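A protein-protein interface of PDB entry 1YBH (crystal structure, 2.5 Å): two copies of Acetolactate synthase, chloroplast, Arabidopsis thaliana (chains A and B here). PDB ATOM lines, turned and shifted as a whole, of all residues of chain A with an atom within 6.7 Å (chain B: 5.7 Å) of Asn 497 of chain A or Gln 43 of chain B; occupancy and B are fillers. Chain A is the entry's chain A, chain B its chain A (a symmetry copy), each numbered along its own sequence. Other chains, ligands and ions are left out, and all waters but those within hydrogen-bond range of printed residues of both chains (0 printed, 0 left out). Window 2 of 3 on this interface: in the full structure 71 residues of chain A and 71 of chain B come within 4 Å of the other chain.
The side-chain carboxylate of Glu 40 of chain B lies within hydrogen-bond range of the side-chain hydroxyl of Tyr 494 of chain A (2.6 Å).
The side-chain amide nitrogen (ND2) of Asn 497 of chain A sits at hydrogen-bond distance from the side-chain amide oxygen (OE1) of Gln 43 of chain B.
The side-chain amide nitrogen (ND2) of Asn 497 of chain A is in hydrogen-bond range of the side-chain hydroxyl (OG1) of Thr 46 of chain B, at 3.4 Å.
The backbone carbonyl oxygen (O) of Glu 490 of chain A lies within hydrogen-bond range of the backbone NH (N) of Lys 495 of chain A.
O of Glu 490 of chain A is in hydrogen-bond range of N of Ala 496 of chain A, 3.0 Å away.
The side-chain carboxylate of Glu 490 of chain A lies within salt-bridge range of the guanidinium group of Arg 498 of chain A (3.3 Å).
The guanidinium group (NH2) of Arg 498 of chain A is in salt-bridge range of the side-chain carboxylate (OD1) of Asp 491 of chain A (2.9 Å).
NH1 of Arg 498 of chain A sits at hydrogen-bond distance from O of Ala 496 of chain A (3.2 Å).
The side-chain hydroxyl (OG1) of Thr 46 of chain B lies within hydrogen-bond range of the backbone carbonyl oxygen (O) of Gln 43 of chain B (2.7 Å).
Among the printed residues, merely in contact across the chains: Glu 490 of chain A with Met 39 of chain B (3.7 Å), Glu 490 of chain A with Gln 43 of chain B (3.8 Å), Tyr 494 of chain A with Met 39 of chain B (3.7 Å), Tyr 494 of chain A with Gln 43 of chain B (3.5 Å), Arg 498 of chain A with Thr 46 of chain B (3.96 Å), Ala 499 of chain A with His 42 of chain B (3.9 Å), Ala 499 of chain A with Gln 43 of chain B (3.5 Å), Ala 499 of chain A with Thr 46 of chain B (3.8 Å) and His 500 of chain A with His 42 of chain B (2.8 Å).
Of chain B, only Gln 43 and Thr 46 come within 4 Å of Asn 497 of chain A.
Gln 43 of chain B touches just these residues of chain A: Glu 490, Tyr 494, Asn 497 and Ala 499.
Of the printed residues of chain B, Glu 490 of chain A touches Met 39 and Gln 43.
Printed residues of chain B within 4 Å of Tyr 494 of chain A: Met 39, Glu 40 and Gln 43.
Of the printed residues of chain A, His 42 of chain B touches Ala 499 and His 500.
Of the printed residues of chain A, Met 39 of chain B touches Glu 490 and Tyr 494.
Printed residues of chain B within 4 Å of Ala 499 of chain A: His 42 (3.9 Å), Gln 43 (3.5 Å) and Thr 46 (3.8 Å).
Ala 496 of chain A touches none of the printed residues of chain B.
Of the 10 printed residues of chain A, 6 touch a printed residue of chain B.
Hydrophobic or aromatic side chains of chain A within 4 Å of the printed part of chain B: Tyr 494, Ala 499 and His 500.
Of the 10 printed residues of chain B, 5 touch a printed residue of chain A.
Printed residues of chain B that touch a printed residue of chain A: Met 39, Glu 40, His 42, Gln 43 and Thr 46.
Hydrophobic or aromatic side chains of chain B within 4 Å of the printed part of chain A: Met 39 and His 42.
No position is printed for both chains.
Of the 12 pairs that touch across the chains among the printed residues, none has its exchanged pair printed and touching as well.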
ATOM      1  N   GLU A 490      -0.180   0.164 -11.785  1.00  0.00           N
ATOM      2  CA  GLU A 490      -1.399  -0.478 -11.311  1.00  0.00           C
ATOM      3  C   GLU A 490      -1.178  -0.815  -9.840  1.00  0.00           C
ATOM      4  O   GLU A 490      -2.041  -0.567  -9.002  1.00  0.00           O
ATOM      5  CB  GLU A 490      -1.705  -1.752 -12.112  1.00  0.00           C
ATOM      6  CG  GLU A 490      -2.068  -1.489 -13.569  1.00  0.00           C
ATOM      7  CD  GLU A 490      -2.439  -2.756 -14.351  1.00  0.00           C
ATOM      8  OE1 GLU A 490      -1.754  -3.795 -14.182  1.00  0.00           O
ATOM      9  OE2 GLU A 490      -3.407  -2.701 -15.149  1.00  0.00           O
ATOM     10  N   ASP A 491      -0.002  -1.354  -9.527  1.00  0.00           N
ATOM     11  CA  ASP A 491       0.328  -1.707  -8.152  1.00  0.00           C
ATOM     12  C   ASP A 491       0.291  -0.482  -7.238  1.00  0.00           C
ATOM     13  O   ASP A 491      -0.384  -0.486  -6.209  1.00  0.00           O
ATOM     14  CB  ASP A 491       1.721  -2.350  -8.069  1.00  0.00           C
ATOM     15  CG  ASP A 491       1.801  -3.699  -8.779  1.00  0.00           C
ATOM     16  OD1 ASP A 491       0.737  -4.296  -9.053  1.00  0.00           O
ATOM     17  OD2 ASP A 491       2.930  -4.169  -9.052  1.00  0.00           O
ATOM     18  N   TYR A 494      -3.486   1.691  -8.278  1.00  0.00           N
ATOM     19  CA  TYR A 494      -4.757   1.028  -8.539  1.00  0.00           C
ATOM     20  C   TYR A 494      -4.966  -0.283  -7.786  1.00  0.00           C
ATOM     21  O   TYR A 494      -5.707  -1.158  -8.240  1.00  0.00           O
ATOM     22  CB  TYR A 494      -4.929   0.812 -10.041  1.00  0.00           C
ATOM     23  CG  TYR A 494      -4.943   2.111 -10.815  1.00  0.00           C
ATOM     24  CD1 TYR A 494      -3.761   2.667 -11.310  1.00  0.00           C
ATOM     25  CD2 TYR A 494      -6.135   2.811 -11.015  1.00  0.00           C
ATOM     26  CE1 TYR A 494      -3.766   3.886 -11.984  1.00  0.00           C
ATOM     27  CE2 TYR A 494      -6.152   4.031 -11.685  1.00  0.00           C
ATOM     28  CZ  TYR A 494      -4.964   4.565 -12.170  1.00  0.00           C
ATOM     29  OH  TYR A 494      -4.977   5.771 -12.842  1.00  0.00           O
ATOM     30  N   LYS A 495      -4.317  -0.402  -6.627  1.00  0.00           N
ATOM     31  CA  LYS A 495      -4.438  -1.589  -5.790  1.00  0.00           C
ATOM     32  C   LYS A 495      -4.174  -2.851  -6.593  1.00  0.00           C
ATOM     33  O   LYS A 495      -4.899  -3.838  -6.471  1.00  0.00           O
ATOM     34  CB  LYS A 495      -5.837  -1.658  -5.188  1.00  0.00           C
ATOM     35  CG  LYS A 495      -6.219  -0.448  -4.357  1.00  0.00           C
ATOM     36  CD  LYS A 495      -7.731  -0.344  -4.254  1.00  0.00           C
ATOM     37  CE  LYS A 495      -8.168   0.892  -3.485  1.00  0.00           C
ATOM     38  NZ  LYS A 495      -9.653   1.068  -3.548  1.00  0.00           N
ATOM     39  N   ALA A 496      -3.144  -2.806  -7.429  1.00  0.00           N
ATOM     40  CA  ALA A 496      -2.762  -3.944  -8.250  1.00  0.00           C
ATOM     41  C   ALA A 496      -3.889  -4.541  -9.106  1.00  0.00           C
ATOM     42  O   ALA A 496      -3.806  -5.697  -9.524  1.00  0.00           O
ATOM     43  CB  ALA A 496      -2.147  -5.017  -7.373  1.00  0.00           C
ATOM     44  N   ASN A 497      -4.937  -3.769  -9.373  1.00  0.00           N
ATOM     45  CA  ASN A 497      -6.016  -4.275 -10.214  1.00  0.00           C
ATOM     46  C   ASN A 497      -5.528  -4.372 -11.670  1.00  0.00           C
ATOM     47  O   ASN A 497      -5.404  -3.360 -12.362  1.00  0.00           O
ATOM     48  CB  ASN A 497      -7.236  -3.358 -10.138  1.00  0.00           C
ATOM     49  CG  ASN A 497      -8.382  -3.853 -11.001  1.00  0.00           C
ATOM     50  OD1 ASN A 497      -8.786  -5.015 -10.906  1.00  0.00           O
ATOM     51  ND2 ASN A 497      -8.913  -2.975 -11.850  1.00  0.00           N
ATOM     52  N   ARG A 498      -5.248  -5.587 -12.128  1.00  0.00           N
ATOM     53  CA  ARG A 498      -4.758  -5.795 -13.489  1.00  0.00           C
ATOM     54  C   ARG A 498      -5.753  -5.447 -14.581  1.00  0.00           C
ATOM     55  O   ARG A 498      -6.887  -5.925 -14.580  1.00  0.00           O
ATOM     56  CB  ARG A 498      -4.313  -7.246 -13.678  1.00  0.00           C
ATOM     57  CG  ARG A 498      -3.097  -7.616 -12.860  1.00  0.00           C
ATOM     58  CD  ARG A 498      -1.831  -6.999 -13.413  1.00  0.00           C
ATOM     59  NE  ARG A 498      -0.730  -7.190 -12.479  1.00  0.00           N
ATOM     60  CZ  ARG A 498      -0.450  -6.368 -11.471  1.00  0.00           C
ATOM     61  NH1 ARG A 498      -1.184  -5.281 -11.268  1.00  0.00           N
ATOM     62  NH2 ARG A 498       0.540  -6.659 -10.641  1.00  0.00           N
ATOM     63  N   ALA A 499      -5.320  -4.619 -15.526  1.00  0.00           N
ATOM     64  CA  ALA A 499      -6.180  -4.235 -16.627  1.00  0.00           C
ATOM     65  C   ALA A 499      -5.480  -4.451 -17.968  1.00  0.00           C
ATOM     66  O   ALA A 499      -4.879  -3.539 -18.534  1.00  0.00           O
ATOM     67  CB  ALA A 499      -6.620  -2.780 -16.474  1.00  0.00           C
ATOM     68  N   HIS A 500      -5.548  -5.683 -18.460  1.00  0.00           N
ATOM     69  CA  HIS A 500      -4.963  -6.042 -19.744  1.00  0.00           C
ATOM     70  C   HIS A 500      -3.453  -5.832 -19.802  1.00  0.00           C
ATOM     71  O   HIS A 500      -2.918  -5.443 -20.839  1.00  0.00           O
ATOM     72  CB  HIS A 500      -5.644  -5.226 -20.840  1.00  0.00           C
ATOM     73  CG  HIS A 500      -7.073  -4.903 -20.538  1.00  0.00           C
ATOM     74  ND1 HIS A 500      -8.032  -5.875 -20.356  1.00  0.00           N
ATOM     75  CD2 HIS A 500      -7.699  -3.719 -20.352  1.00  0.00           C
ATOM     76  CE1 HIS A 500      -9.188  -5.304 -20.074  1.00  0.00           C
ATOM     77  NE2 HIS A 500      -9.014  -3.995 -20.065  1.00  0.00           N
ATOM     78  N   THR A 501      -2.758  -6.093 -18.701  1.00  0.00           N
ATOM     79  CA  THR A 501      -1.315  -5.912 -18.705  1.00  0.00           C
ATOM     80  C   THR A 501      -0.524  -7.214 -18.752  1.00  0.00           C
ATOM     81  O   THR A 501       0.704  -7.193 -18.861  1.00  0.00           O
ATOM     82  CB  THR A 501      -0.856  -5.089 -17.493  1.00  0.00           C
ATOM     83  OG1 THR A 501      -1.283  -5.732 -16.288  1.00  0.00           O
ATOM     84  CG2 THR A 501      -1.444  -3.681 -17.558  1.00  0.00           C
ATOM     85  N   SER B  38      -3.976   6.189 -20.832  1.00  0.00           N
ATOM     86  CA  SER B  38      -5.293   5.574 -20.950  1.00  0.00           C
ATOM     87  C   SER B  38      -5.604   4.568 -19.831  1.00  0.00           C
ATOM     88  O   SER B  38      -6.632   3.880 -19.872  1.00  0.00           O
ATOM     89  CB  SER B  38      -5.429   4.888 -22.314  1.00  0.00           C
ATOM     90  OG  SER B  38      -4.597   3.743 -22.407  1.00  0.00           O
ATOM     91  N   MET B  39      -4.731   4.493 -18.828  1.00  0.00           N
ATOM     92  CA  MET B  39      -4.928   3.564 -17.717  1.00  0.00           C
ATOM     93  C   MET B  39      -6.300   3.659 -17.067  1.00  0.00           C
ATOM     94  O   MET B  39      -6.914   2.642 -16.757  1.00  0.00           O
ATOM     95  CB  MET B  39      -3.864   3.775 -16.647  1.00  0.00           C
ATOM     96  CG  MET B  39      -2.531   3.181 -17.000  1.00  0.00           C
ATOM     97  SD  MET B  39      -1.397   3.389 -15.644  1.00  0.00           S
ATOM     98  CE  MET B  39      -1.945   2.023 -14.574  1.00  0.00           C
ATOM     99  N   GLU B  40      -6.776   4.878 -16.842  1.00  0.00           N
ATOM    100  CA  GLU B  40      -8.081   5.068 -16.229  1.00  0.00           C
ATOM    101  C   GLU B  40      -9.149   4.388 -17.077  1.00  0.00           C
ATOM    102  O   GLU B  40     -10.024   3.701 -16.560  1.00  0.00           O
ATOM    103  CB  GLU B  40      -8.407   6.555 -16.101  1.00  0.00           C
ATOM    104  CG  GLU B  40      -7.620   7.309 -15.042  1.00  0.00           C
ATOM    105  CD  GLU B  40      -8.017   6.931 -13.626  1.00  0.00           C
ATOM    106  OE1 GLU B  40      -9.175   6.500 -13.423  1.00  0.00           O
ATOM    107  OE2 GLU B  40      -7.176   7.086 -12.714  1.00  0.00           O
ATOM    108  N   ILE B  41      -9.076   4.578 -18.388  1.00  0.00           N
ATOM    109  CA  ILE B  41     -10.063   3.975 -19.269  1.00  0.00           C
ATOM    110  C   ILE B  41     -10.023   2.457 -19.154  1.00  0.00           C
ATOM    111  O   ILE B  41     -11.071   1.804 -19.130  1.00  0.00           O
ATOM    112  CB  ILE B  41      -9.843   4.415 -20.735  1.00  0.00           C
ATOM    113  CG1 ILE B  41     -10.112   5.926 -20.852  1.00  0.00           C
ATOM    114  CG2 ILE B  41     -10.750   3.614 -21.668  1.00  0.00           C
ATOM    115  CD1 ILE B  41      -9.896   6.502 -22.244  1.00  0.00           C
ATOM    116  N   HIS B  42      -8.819   1.893 -19.065  1.00  0.00           N
ATOM    117  CA  HIS B  42      -8.694   0.451 -18.939  1.00  0.00           C
ATOM    118  C   HIS B  42      -9.255  -0.032 -17.604  1.00  0.00           C
ATOM    119  O   HIS B  42      -9.935  -1.061 -17.552  1.00  0.00           O
ATOM    120  CB  HIS B  42      -7.235   0.026 -19.119  1.00  0.00           C
ATOM    121  CG  HIS B  42      -6.825  -0.070 -20.555  1.00  0.00           C
ATOM    122  ND1 HIS B  42      -7.014  -1.209 -21.305  1.00  0.00           N
ATOM    123  CD2 HIS B  42      -6.336   0.862 -21.407  1.00  0.00           C
ATOM    124  CE1 HIS B  42      -6.663  -0.975 -22.557  1.00  0.00           C
ATOM    125  NE2 HIS B  42      -6.247   0.277 -22.646  1.00  0.00           N
ATOM    126  N   GLN B  43      -8.991   0.714 -16.531  1.00  0.00           N
ATOM    127  CA  GLN B  43      -9.507   0.345 -15.218  1.00  0.00           C
ATOM    128  C   GLN B  43     -11.040   0.313 -15.261  1.00  0.00           C
ATOM    129  O   GLN B  43     -11.661  -0.641 -14.787  1.00  0.00           O
ATOM    130  CB  GLN B  43      -9.044   1.338 -14.146  1.00  0.00           C
ATOM    131  CG  GLN B  43      -7.574   1.247 -13.787  1.00  0.00           C
ATOM    132  CD  GLN B  43      -7.228  -0.050 -13.086  1.00  0.00           C
ATOM    133  OE1 GLN B  43      -7.849  -0.405 -12.090  1.00  0.00           O
ATOM    134  NE2 GLN B  43      -6.228  -0.760 -13.595  1.00  0.00           N
ATOM    135  N   ALA B  44     -11.645   1.349 -15.844  1.00  0.00           N
ATOM    136  CA  ALA B  44     -13.103   1.429 -15.945  1.00  0.00           C
ATOM    137  C   ALA B  44     -13.641   0.293 -16.802  1.00  0.00           C
ATOM    138  O   ALA B  44     -14.759  -0.177 -16.611  1.00  0.00           O
ATOM    139  CB  ALA B  44     -13.526   2.771 -16.547  1.00  0.00           C
ATOM    140  N   LEU B  45     -12.836  -0.143 -17.752  1.00  0.00           N
ATOM    141  CA  LEU B  45     -13.230  -1.213 -18.642  1.00  0.00           C
ATOM    142  C   LEU B  45     -13.408  -2.525 -17.872  1.00  0.00           C
ATOM    143  O   LEU B  45     -14.343  -3.282 -18.136  1.00  0.00           O
ATOM    144  CB  LEU B  45     -12.169  -1.367 -19.724  1.00  0.00           C
ATOM    145  CG  LEU B  45     -12.572  -1.279 -21.194  1.00  0.00           C
ATOM    146  CD1 LEU B  45     -13.813  -0.447 -21.364  1.00  0.00           C
ATOM    147  CD2 LEU B  45     -11.404  -0.707 -21.983  1.00  0.00           C
ATOM    148  N   THR B  46     -12.527  -2.789 -16.912  1.00  0.00           N
ATOM    149  CA  THR B  46     -12.618  -4.023 -16.137  1.00  0.00           C
ATOM    150  C   THR B  46     -13.839  -4.046 -15.220  1.00  0.00           C
ATOM    151  O   THR B  46     -14.211  -5.099 -14.712  1.00  0.00           O
ATOM    152  CB  THR B  46     -11.365  -4.262 -15.263  1.00  0.00           C
ATOM    153  OG1 THR B  46     -11.320  -3.293 -14.210  1.00  0.00           O
ATOM    154  CG2 THR B  46     -10.101  -4.171 -16.097  1.00  0.00           C
ATOM    155  N   ARG B  47     -14.460  -2.893 -14.998  1.00  0.00           N
ATOM    156  CA  ARG B  47     -15.643  -2.843 -14.145  1.00  0.00           C
ATOM    157  C   ARG B  47     -16.879  -3.120 -14.970  1.00  0.00           C
ATOM    158  O   ARG B  47     -17.954  -3.367 -14.431  1.00  0.00           O
ATOM    159  CB  ARG B  47     -15.782  -1.480 -13.473  1.00  0.00           C
ATOM    160  CG  ARG B  47     -14.720  -1.205 -12.439  1.00  0.00           C
ATOM    161  CD  ARG B  47     -14.769   0.234 -12.005  1.00  0.00           C
ATOM    162  NE  ARG B  47     -13.436   0.705 -11.659  1.00  0.00           N
ATOM    163  CZ  ARG B  47     -12.933   1.855 -12.083  1.00  0.00           C
ATOM    164  NH1 ARG B  47     -13.662   2.641 -12.867  1.00  0.00           N
ATOM    165  NH2 ARG B  47     -11.704   2.217 -11.733  1.00  0.00           N
